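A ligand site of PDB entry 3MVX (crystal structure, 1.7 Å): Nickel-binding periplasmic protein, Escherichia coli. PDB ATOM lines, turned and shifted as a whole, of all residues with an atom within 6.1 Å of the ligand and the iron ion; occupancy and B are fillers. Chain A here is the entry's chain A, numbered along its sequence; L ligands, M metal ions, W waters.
Tyr 22 touches the ligand.
CE of Met 27 touches O5 of the ligand, at 3.5 Å.
Trp 100 touches the ligand.
Trp 398 touches the ligand.
His 416 touches the ligand (NE2 to C2, 3.5 Å).
CG2 of Thr 490 touches C14 of the ligand, 3.6 Å away.
Of the 20 residues printed, 8 come within 4 Å of the ligand.
OH of Tyr 22 lies within hydrogen-bond range of NE1 of Trp 100.
No residue comes within 4 Å of the iron ion.
Water W3 lies within hydrogen-bond range of OH of Tyr 402, O5 of the ligand and O of Arg 137.
Water W4 bridges the backbone NH of Thr 23 (3.1 Å) and an oxygen (O3) of the ligand (3.4 Å).
Water W2 bridges the backbone carbonyl oxygen (O) of Arg 396 (2.8 Å) and the indole nitrogen (NE1) of Trp 398 (3.0 Å).
An oxygen (O1) of the ligand binds the iron ion, 2.0 Å away.
The iron ion is bound by an oxygen (O2) of the ligand (2.1 Å).
O4 of the ligand is bound to the iron ion.
The iron ion is bound by N1 of the ligand.
The iron ion is bound by water W5 (2.2 Å).
The iron ion is bound by N2 of the ligand (2.3 Å).
The guanidinium group of Arg 97 is in salt-bridge range of an oxygen (O3) of the ligand (2.8 Å).
NE of Arg 137 is in salt-bridge range of O5 of the ligand (2.8 Å).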
ATOM      1  N   TYR A  22       7.372  -6.597  36.176  1.00  0.00           N
ATOM      2  CA  TYR A  22       7.109  -6.429  34.782  1.00  0.00           C
ATOM      3  C   TYR A  22       7.963  -5.327  34.173  1.00  0.00           C
ATOM      4  O   TYR A  22       9.024  -5.127  34.658  1.00  0.00           O
ATOM      5  CB  TYR A  22       5.612  -6.240  34.526  1.00  0.00           C
ATOM      6  CG  TYR A  22       4.831  -7.420  35.066  1.00  0.00           C
ATOM      7  CD1 TYR A  22       4.443  -7.489  36.380  1.00  0.00           C
ATOM      8  CD2 TYR A  22       4.523  -8.493  34.276  1.00  0.00           C
ATOM      9  CE1 TYR A  22       3.769  -8.547  36.842  1.00  0.00           C
ATOM     10  CE2 TYR A  22       3.855  -9.578  34.771  1.00  0.00           C
ATOM     11  CZ  TYR A  22       3.462  -9.623  36.029  1.00  0.00           C
ATOM     12  OH  TYR A  22       2.804 -10.726  36.518  1.00  0.00           O
ATOM     13  N   THR A  23       7.507  -4.627  33.124  1.00  0.00           N
ATOM     14  CA  THR A  23       8.371  -3.625  32.548  1.00  0.00           C
ATOM     15  C   THR A  23       8.923  -2.663  33.651  1.00  0.00           C
ATOM     16  O   THR A  23       8.193  -2.271  34.559  1.00  0.00           O
ATOM     17  CB  THR A  23       7.604  -2.867  31.395  1.00  0.00           C
ATOM     18  OG1 THR A  23       8.549  -2.015  30.739  1.00  0.00           O
ATOM     19  CG2 THR A  23       6.479  -2.028  32.026  1.00  0.00           C
ATOM     20  N   MET A  27      11.198  -9.881  29.316  1.00  0.00           N
ATOM     21  CA  MET A  27      10.787 -11.257  29.540  1.00  0.00           C
ATOM     22  C   MET A  27      11.835 -12.280  29.119  1.00  0.00           C
ATOM     23  O   MET A  27      11.938 -13.349  29.719  1.00  0.00           O
ATOM     24  CB  MET A  27       9.467 -11.542  28.827  1.00  0.00           C
ATOM     25  CG  MET A  27       8.294 -10.718  29.348  1.00  0.00           C
ATOM     26  SD  MET A  27       6.762 -11.056  28.460  1.00  0.00           S
ATOM     27  CE  MET A  27       6.449 -12.745  28.945  1.00  0.00           C
ATOM     28  N   ARG A  97      -1.194  -7.296  41.355  1.00  0.00           N
ATOM     29  CA  ARG A  97      -0.447  -6.991  40.080  1.00  0.00           C
ATOM     30  C   ARG A  97      -0.449  -8.107  39.041  1.00  0.00           C
ATOM     31  O   ARG A  97      -0.217  -7.862  37.873  1.00  0.00           O
ATOM     32  CB  ARG A  97       1.005  -6.632  40.473  1.00  0.00           C
ATOM     33  CG  ARG A  97       1.923  -6.140  39.360  1.00  0.00           C
ATOM     34  CD  ARG A  97       1.294  -4.988  38.649  1.00  0.00           C
ATOM     35  NE  ARG A  97       2.103  -4.479  37.532  1.00  0.00           N
ATOM     36  CZ  ARG A  97       2.059  -4.966  36.262  1.00  0.00           C
ATOM     37  NH1 ARG A  97       1.254  -6.002  35.986  1.00  0.00           N
ATOM     38  NH2 ARG A  97       2.798  -4.383  35.260  1.00  0.00           N
ATOM     39  N   TRP A 100      -3.863 -10.518  35.691  1.00  0.00           N
ATOM     40  CA  TRP A 100      -3.990 -11.002  34.296  1.00  0.00           C
ATOM     41  C   TRP A 100      -3.760 -12.535  34.164  1.00  0.00           C
ATOM     42  O   TRP A 100      -4.223 -13.146  33.216  1.00  0.00           O
ATOM     43  CB  TRP A 100      -2.959 -10.314  33.408  1.00  0.00           C
ATOM     44  CG  TRP A 100      -1.521 -10.704  33.749  1.00  0.00           C
ATOM     45  CD1 TRP A 100      -0.673 -10.136  34.703  1.00  0.00           C
ATOM     46  CD2 TRP A 100      -0.775 -11.737  33.136  1.00  0.00           C
ATOM     47  NE1 TRP A 100       0.537 -10.770  34.700  1.00  0.00           N
ATOM     48  CE2 TRP A 100       0.508 -11.777  33.785  1.00  0.00           C
ATOM     49  CE3 TRP A 100      -1.056 -12.676  32.134  1.00  0.00           C
ATOM     50  CZ2 TRP A 100       1.520 -12.691  33.407  1.00  0.00           C
ATOM     51  CZ3 TRP A 100      -0.082 -13.632  31.770  1.00  0.00           C
ATOM     52  CH2 TRP A 100       1.177 -13.660  32.409  1.00  0.00           C
ATOM     53  N   PRO A 136       7.699 -17.301  31.741  1.00  0.00           N
ATOM     54  CA  PRO A 136       8.929 -16.533  32.086  1.00  0.00           C
ATOM     55  C   PRO A 136       8.722 -15.842  33.461  1.00  0.00           C
ATOM     56  O   PRO A 136       9.736 -15.679  34.153  1.00  0.00           O
ATOM     57  CB  PRO A 136       8.971 -15.424  30.993  1.00  0.00           C
ATOM     58  CG  PRO A 136       8.403 -16.260  29.724  1.00  0.00           C
ATOM     59  CD  PRO A 136       7.238 -17.060  30.339  1.00  0.00           C
ATOM     60  N   ARG A 137       7.494 -15.351  33.789  1.00  0.00           N
ATOM     61  CA  ARG A 137       7.268 -14.634  35.059  1.00  0.00           C
ATOM     62  C   ARG A 137       5.801 -14.804  35.348  1.00  0.00           C
ATOM     63  O   ARG A 137       4.998 -14.968  34.378  1.00  0.00           O
ATOM     64  CB  ARG A 137       7.693 -13.145  34.966  1.00  0.00           C
ATOM     65  CG  ARG A 137       6.921 -12.327  33.902  1.00  0.00           C
ATOM     66  CD  ARG A 137       7.638 -11.039  33.591  1.00  0.00           C
ATOM     67  NE  ARG A 137       6.903 -10.236  32.586  1.00  0.00           N
ATOM     68  CZ  ARG A 137       7.369  -9.122  32.078  1.00  0.00           C
ATOM     69  NH1 ARG A 137       8.640  -8.754  32.302  1.00  0.00           N
ATOM     70  NH2 ARG A 137       6.577  -8.393  31.252  1.00  0.00           N
ATOM     71  N   PRO A 138       5.385 -14.719  36.602  1.00  0.00           N
ATOM     72  CA  PRO A 138       6.242 -14.374  37.736  1.00  0.00           C
ATOM     73  C   PRO A 138       6.742 -15.577  38.563  1.00  0.00           C
ATOM     74  O   PRO A 138       7.399 -15.318  39.571  1.00  0.00           O
ATOM     75  CB  PRO A 138       5.241 -13.537  38.577  1.00  0.00           C
ATOM     76  CG  PRO A 138       3.905 -14.340  38.435  1.00  0.00           C
ATOM     77  CD  PRO A 138       3.951 -14.745  36.957  1.00  0.00           C
ATOM     78  N   GLU A 247       2.206 -16.148  16.306  1.00  0.00           N
ATOM     79  CA  GLU A 247       1.060 -15.457  16.998  1.00  0.00           C
ATOM     80  C   GLU A 247       0.358 -14.580  15.989  1.00  0.00           C
ATOM     81  O   GLU A 247       0.851 -14.388  14.826  1.00  0.00           O
ATOM     82  CB  GLU A 247       1.512 -14.593  18.194  1.00  0.00           C
ATOM     83  CG  GLU A 247       2.401 -13.336  17.761  1.00  0.00           C
ATOM     84  CD  GLU A 247       3.411 -12.976  18.855  1.00  0.00           C
ATOM     85  OE1 GLU A 247       3.937 -11.836  18.748  1.00  0.00           O
ATOM     86  OE2 GLU A 247       3.710 -13.815  19.751  1.00  0.00           O
ATOM     87  N   GLN A 385      -5.865   1.556  25.435  1.00  0.00           N
ATOM     88  CA  GLN A 385      -6.220   0.109  25.517  1.00  0.00           C
ATOM     89  C   GLN A 385      -6.967  -0.160  26.837  1.00  0.00           C
ATOM     90  O   GLN A 385      -7.922  -0.918  26.867  1.00  0.00           O
ATOM     91  CB  GLN A 385      -4.958  -0.729  25.517  1.00  0.00           C
ATOM     92  CG  GLN A 385      -4.379  -0.776  24.107  1.00  0.00           C
ATOM     93  CD  GLN A 385      -3.113  -1.612  24.021  1.00  0.00           C
ATOM     94  OE1 GLN A 385      -2.497  -1.685  22.978  1.00  0.00           O
ATOM     95  NE2 GLN A 385      -2.723  -2.203  25.101  1.00  0.00           N
ATOM     96  N   HIS A 395      -3.390  -4.788  17.852  1.00  0.00           N
ATOM     97  CA  HIS A 395      -3.238  -5.712  19.007  1.00  0.00           C
ATOM     98  C   HIS A 395      -2.594  -6.969  18.492  1.00  0.00           C
ATOM     99  O   HIS A 395      -2.368  -7.141  17.291  1.00  0.00           O
ATOM    100  CB  HIS A 395      -4.674  -5.959  19.592  1.00  0.00           C
ATOM    101  CG  HIS A 395      -4.681  -6.587  20.953  1.00  0.00           C
ATOM    102  ND1 HIS A 395      -3.630  -6.474  21.878  1.00  0.00           N
ATOM    103  CD2 HIS A 395      -5.673  -7.277  21.584  1.00  0.00           C
ATOM    104  CE1 HIS A 395      -3.964  -7.150  22.959  1.00  0.00           C
ATOM    105  NE2 HIS A 395      -5.206  -7.626  22.831  1.00  0.00           N
ATOM    106  N   ARG A 396      -2.256  -7.898  19.424  1.00  0.00           N
ATOM    107  CA  ARG A 396      -1.676  -9.180  18.966  1.00  0.00           C
ATOM    108  C   ARG A 396      -1.887 -10.185  20.065  1.00  0.00           C
ATOM    109  O   ARG A 396      -2.093  -9.801  21.207  1.00  0.00           O
ATOM    110  CB  ARG A 396      -0.126  -9.045  18.701  1.00  0.00           C
ATOM    111  CG  ARG A 396       0.685  -8.599  19.930  1.00  0.00           C
ATOM    112  CD  ARG A 396       2.102  -8.029  19.581  1.00  0.00           C
ATOM    113  NE  ARG A 396       2.871  -8.993  18.741  1.00  0.00           N
ATOM    114  CZ  ARG A 396       3.553  -8.651  17.626  1.00  0.00           C
ATOM    115  NH1 ARG A 396       4.209  -9.646  16.952  1.00  0.00           N
ATOM    116  NH2 ARG A 396       3.506  -7.386  17.125  1.00  0.00           N
ATOM    117  N   THR A 397      -1.867 -11.452  19.676  1.00  0.00           N
ATOM    118  CA  THR A 397      -1.924 -12.542  20.686  1.00  0.00           C
ATOM    119  C   THR A 397      -0.519 -12.799  21.194  1.00  0.00           C
ATOM    120  O   THR A 397       0.458 -12.085  20.852  1.00  0.00           O
ATOM    121  CB  THR A 397      -2.557 -13.758  20.160  1.00  0.00           C
ATOM    122  OG1 THR A 397      -1.768 -14.415  19.157  1.00  0.00           O
ATOM    123  CG2 THR A 397      -3.940 -13.374  19.581  1.00  0.00           C
ATOM    124  N   TRP A 398      -0.397 -13.756  22.115  1.00  0.00           N
ATOM    125  CA  TRP A 398       0.782 -13.852  22.956  1.00  0.00           C
ATOM    126  C   TRP A 398       1.726 -15.004  22.636  1.00  0.00           C
ATOM    127  O   TRP A 398       2.776 -15.142  23.264  1.00  0.00           O
ATOM    128  CB  TRP A 398       0.384 -13.909  24.432  1.00  0.00           C
ATOM    129  CG  TRP A 398      -0.277 -12.660  24.916  1.00  0.00           C
ATOM    130  CD1 TRP A 398      -0.323 -11.450  24.282  1.00  0.00           C
ATOM    131  CD2 TRP A 398      -1.004 -12.489  26.145  1.00  0.00           C
ATOM    132  NE1 TRP A 398      -1.030 -10.548  25.038  1.00  0.00           N
ATOM    133  CE2 TRP A 398      -1.455 -11.163  26.190  1.00  0.00           C
ATOM    134  CE3 TRP A 398      -1.301 -13.345  27.212  1.00  0.00           C
ATOM    135  CZ2 TRP A 398      -2.186 -10.650  27.257  1.00  0.00           C
ATOM    136  CZ3 TRP A 398      -2.041 -12.835  28.275  1.00  0.00           C
ATOM    137  CH2 TRP A 398      -2.467 -11.504  28.288  1.00  0.00           C
ATOM    138  N   GLY A 399       1.357 -15.851  21.675  1.00  0.00           N
ATOM    139  CA  GLY A 399       2.230 -16.985  21.344  1.00  0.00           C
ATOM    140  C   GLY A 399       2.144 -18.114  22.373  1.00  0.00           C
ATOM    141  O   GLY A 399       1.544 -17.971  23.427  1.00  0.00           O
ATOM    142  N   TYR A 402       0.893 -19.225  25.896  1.00  0.00           N
ATOM    143  CA  TYR A 402      -0.260 -18.397  26.295  1.00  0.00           C
ATOM    144  C   TYR A 402      -1.495 -18.544  25.417  1.00  0.00           C
ATOM    145  O   TYR A 402      -2.603 -18.306  25.886  1.00  0.00           O
ATOM    146  CB  TYR A 402       0.112 -16.903  26.212  1.00  0.00           C
ATOM    147  CG  TYR A 402       1.259 -16.442  27.032  1.00  0.00           C
ATOM    148  CD1 TYR A 402       2.566 -16.435  26.466  1.00  0.00           C
ATOM    149  CD2 TYR A 402       1.069 -15.951  28.351  1.00  0.00           C
ATOM    150  CE1 TYR A 402       3.724 -16.049  27.244  1.00  0.00           C
ATOM    151  CE2 TYR A 402       2.233 -15.523  29.111  1.00  0.00           C
ATOM    152  CZ  TYR A 402       3.479 -15.577  28.548  1.00  0.00           C
ATOM    153  OH  TYR A 402       4.571 -15.162  29.298  1.00  0.00           O
ATOM    154  N   HIS A 416      -7.746  -4.311  30.201  1.00  0.00           N
ATOM    155  CA  HIS A 416      -7.045  -4.904  29.062  1.00  0.00           C
ATOM    156  C   HIS A 416      -7.851  -4.495  27.821  1.00  0.00           C
ATOM    157  O   HIS A 416      -9.141  -4.421  27.861  1.00  0.00           O
ATOM    158  CB  HIS A 416      -6.959  -6.479  29.073  1.00  0.00           C
ATOM    159  CG  HIS A 416      -5.733  -7.060  29.771  1.00  0.00           C
ATOM    160  ND1 HIS A 416      -5.196  -6.529  30.946  1.00  0.00           N
ATOM    161  CD2 HIS A 416      -4.981  -8.144  29.487  1.00  0.00           C
ATOM    162  CE1 HIS A 416      -4.146  -7.230  31.318  1.00  0.00           C
ATOM    163  NE2 HIS A 416      -4.007  -8.240  30.468  1.00  0.00           N
ATOM    164  N   ALA A 417      -7.150  -4.392  26.681  1.00  0.00           N
ATOM    165  CA  ALA A 417      -7.850  -3.946  25.456  1.00  0.00           C
ATOM    166  C   ALA A 417      -8.980  -4.878  25.050  1.00  0.00           C
ATOM    167  O   ALA A 417     -10.005  -4.451  24.490  1.00  0.00           O
ATOM    168  CB  ALA A 417      -6.868  -3.830  24.278  1.00  0.00           C
ATOM    169  N   ASP A 418      -8.788  -6.187  25.273  1.00  0.00           N
ATOM    170  CA  ASP A 418      -9.822  -7.129  24.767  1.00  0.00           C
ATOM    171  C   ASP A 418     -11.134  -7.011  25.545  1.00  0.00           C
ATOM    172  O   ASP A 418     -12.221  -7.028  24.970  1.00  0.00           O
ATOM    173  CB  ASP A 418      -9.305  -8.601  24.843  1.00  0.00           C
ATOM    174  CG  ASP A 418      -8.070  -8.712  24.075  1.00  0.00           C
ATOM    175  OD1 ASP A 418      -8.193  -8.883  22.850  1.00  0.00           O
ATOM    176  OD2 ASP A 418      -6.993  -8.534  24.719  1.00  0.00           O
ATOM    177  N   THR A 490       8.326 -15.865  23.698  1.00  0.00           N
ATOM    178  CA  THR A 490       9.049 -14.702  24.250  1.00  0.00           C
ATOM    179  C   THR A 490      10.472 -15.008  24.731  1.00  0.00           C
ATOM    180  O   THR A 490      11.169 -14.098  25.162  1.00  0.00           O
ATOM    181  CB  THR A 490       8.334 -14.086  25.450  1.00  0.00           C
ATOM    182  OG1 THR A 490       8.100 -15.109  26.439  1.00  0.00           O
ATOM    183  CG2 THR A 490       6.936 -13.668  25.052  1.00  0.00           C
HETATM  184  C1  LIG L   1      -0.325  -6.946  28.776  1.00  0.00           C
HETATM  185  C2  LIG L   1      -1.674  -6.779  28.344  1.00  0.00           C
HETATM  186  C3  LIG L   1      -1.917  -6.763  26.953  1.00  0.00           C
HETATM  187  C4  LIG L   1      -0.907  -6.921  26.005  1.00  0.00           C
HETATM  188  C5  LIG L   1       0.423  -7.070  26.462  1.00  0.00           C
HETATM  189  C6  LIG L   1       0.709  -7.071  27.873  1.00  0.00           C
HETATM  190  O1  LIG L   1       2.051  -7.186  28.206  1.00  0.00           O
HETATM  191  C7  LIG L   1      -0.028  -6.927  30.248  1.00  0.00           C
HETATM  192  N1  LIG L   1       0.831  -8.088  30.645  1.00  0.00           N
HETATM  193  C8  LIG L   1       0.039  -9.277  30.488  1.00  0.00           C
HETATM  194  C9  LIG L   1       0.896 -10.567  30.440  1.00  0.00           C
HETATM  195  N2  LIG L   1       2.030 -10.386  29.432  1.00  0.00           N
HETATM  196  C10 LIG L   1       1.360 -10.667  28.121  1.00  0.00           C
HETATM  197  C11 LIG L   1       2.402 -10.892  27.031  1.00  0.00           C
HETATM  198  C12 LIG L   1       2.629 -12.208  26.535  1.00  0.00           C
HETATM  199  C13 LIG L   1       3.631 -12.365  25.528  1.00  0.00           C
HETATM  200  C14 LIG L   1       4.335 -11.248  25.029  1.00  0.00           C
HETATM  201  C15 LIG L   1       4.071  -9.974  25.539  1.00  0.00           C
HETATM  202  C16 LIG L   1       3.133  -9.805  26.574  1.00  0.00           C
HETATM  203  C17 LIG L   1       1.130  -7.982  32.143  1.00  0.00           C
HETATM  204  C18 LIG L   1       2.155  -6.825  32.173  1.00  0.00           C
HETATM  205  O2  LIG L   1       2.981  -6.832  31.227  1.00  0.00           O
HETATM  206  C19 LIG L   1       3.013 -11.392  29.815  1.00  0.00           C
HETATM  207  O3  LIG L   1       2.101  -6.018  33.151  1.00  0.00           O
HETATM  208  C20 LIG L   1       3.906 -10.756  30.891  1.00  0.00           C
HETATM  209  O4  LIG L   1       3.772  -9.549  31.050  1.00  0.00           O
HETATM  210  O5  LIG L   1       4.557 -11.527  31.651  1.00  0.00           O
HETATM  211 FE    FE M   1       2.743  -8.260  29.717  1.00  0.00          FE
HETATM  212  O   HOH W   1       1.908  -8.884  23.327  1.00  0.00           O
HETATM  213  O   HOH W   2      -0.727  -8.267  23.107  1.00  0.00           O
HETATM  214  O   HOH W   3       4.535 -14.227  31.737  1.00  0.00           O
HETATM  215  O   HOH W   4       4.901  -4.822  31.532  1.00  0.00           O
HETATM  216  O   HOH W   5       4.706  -7.812  28.916  1.00  0.00           O
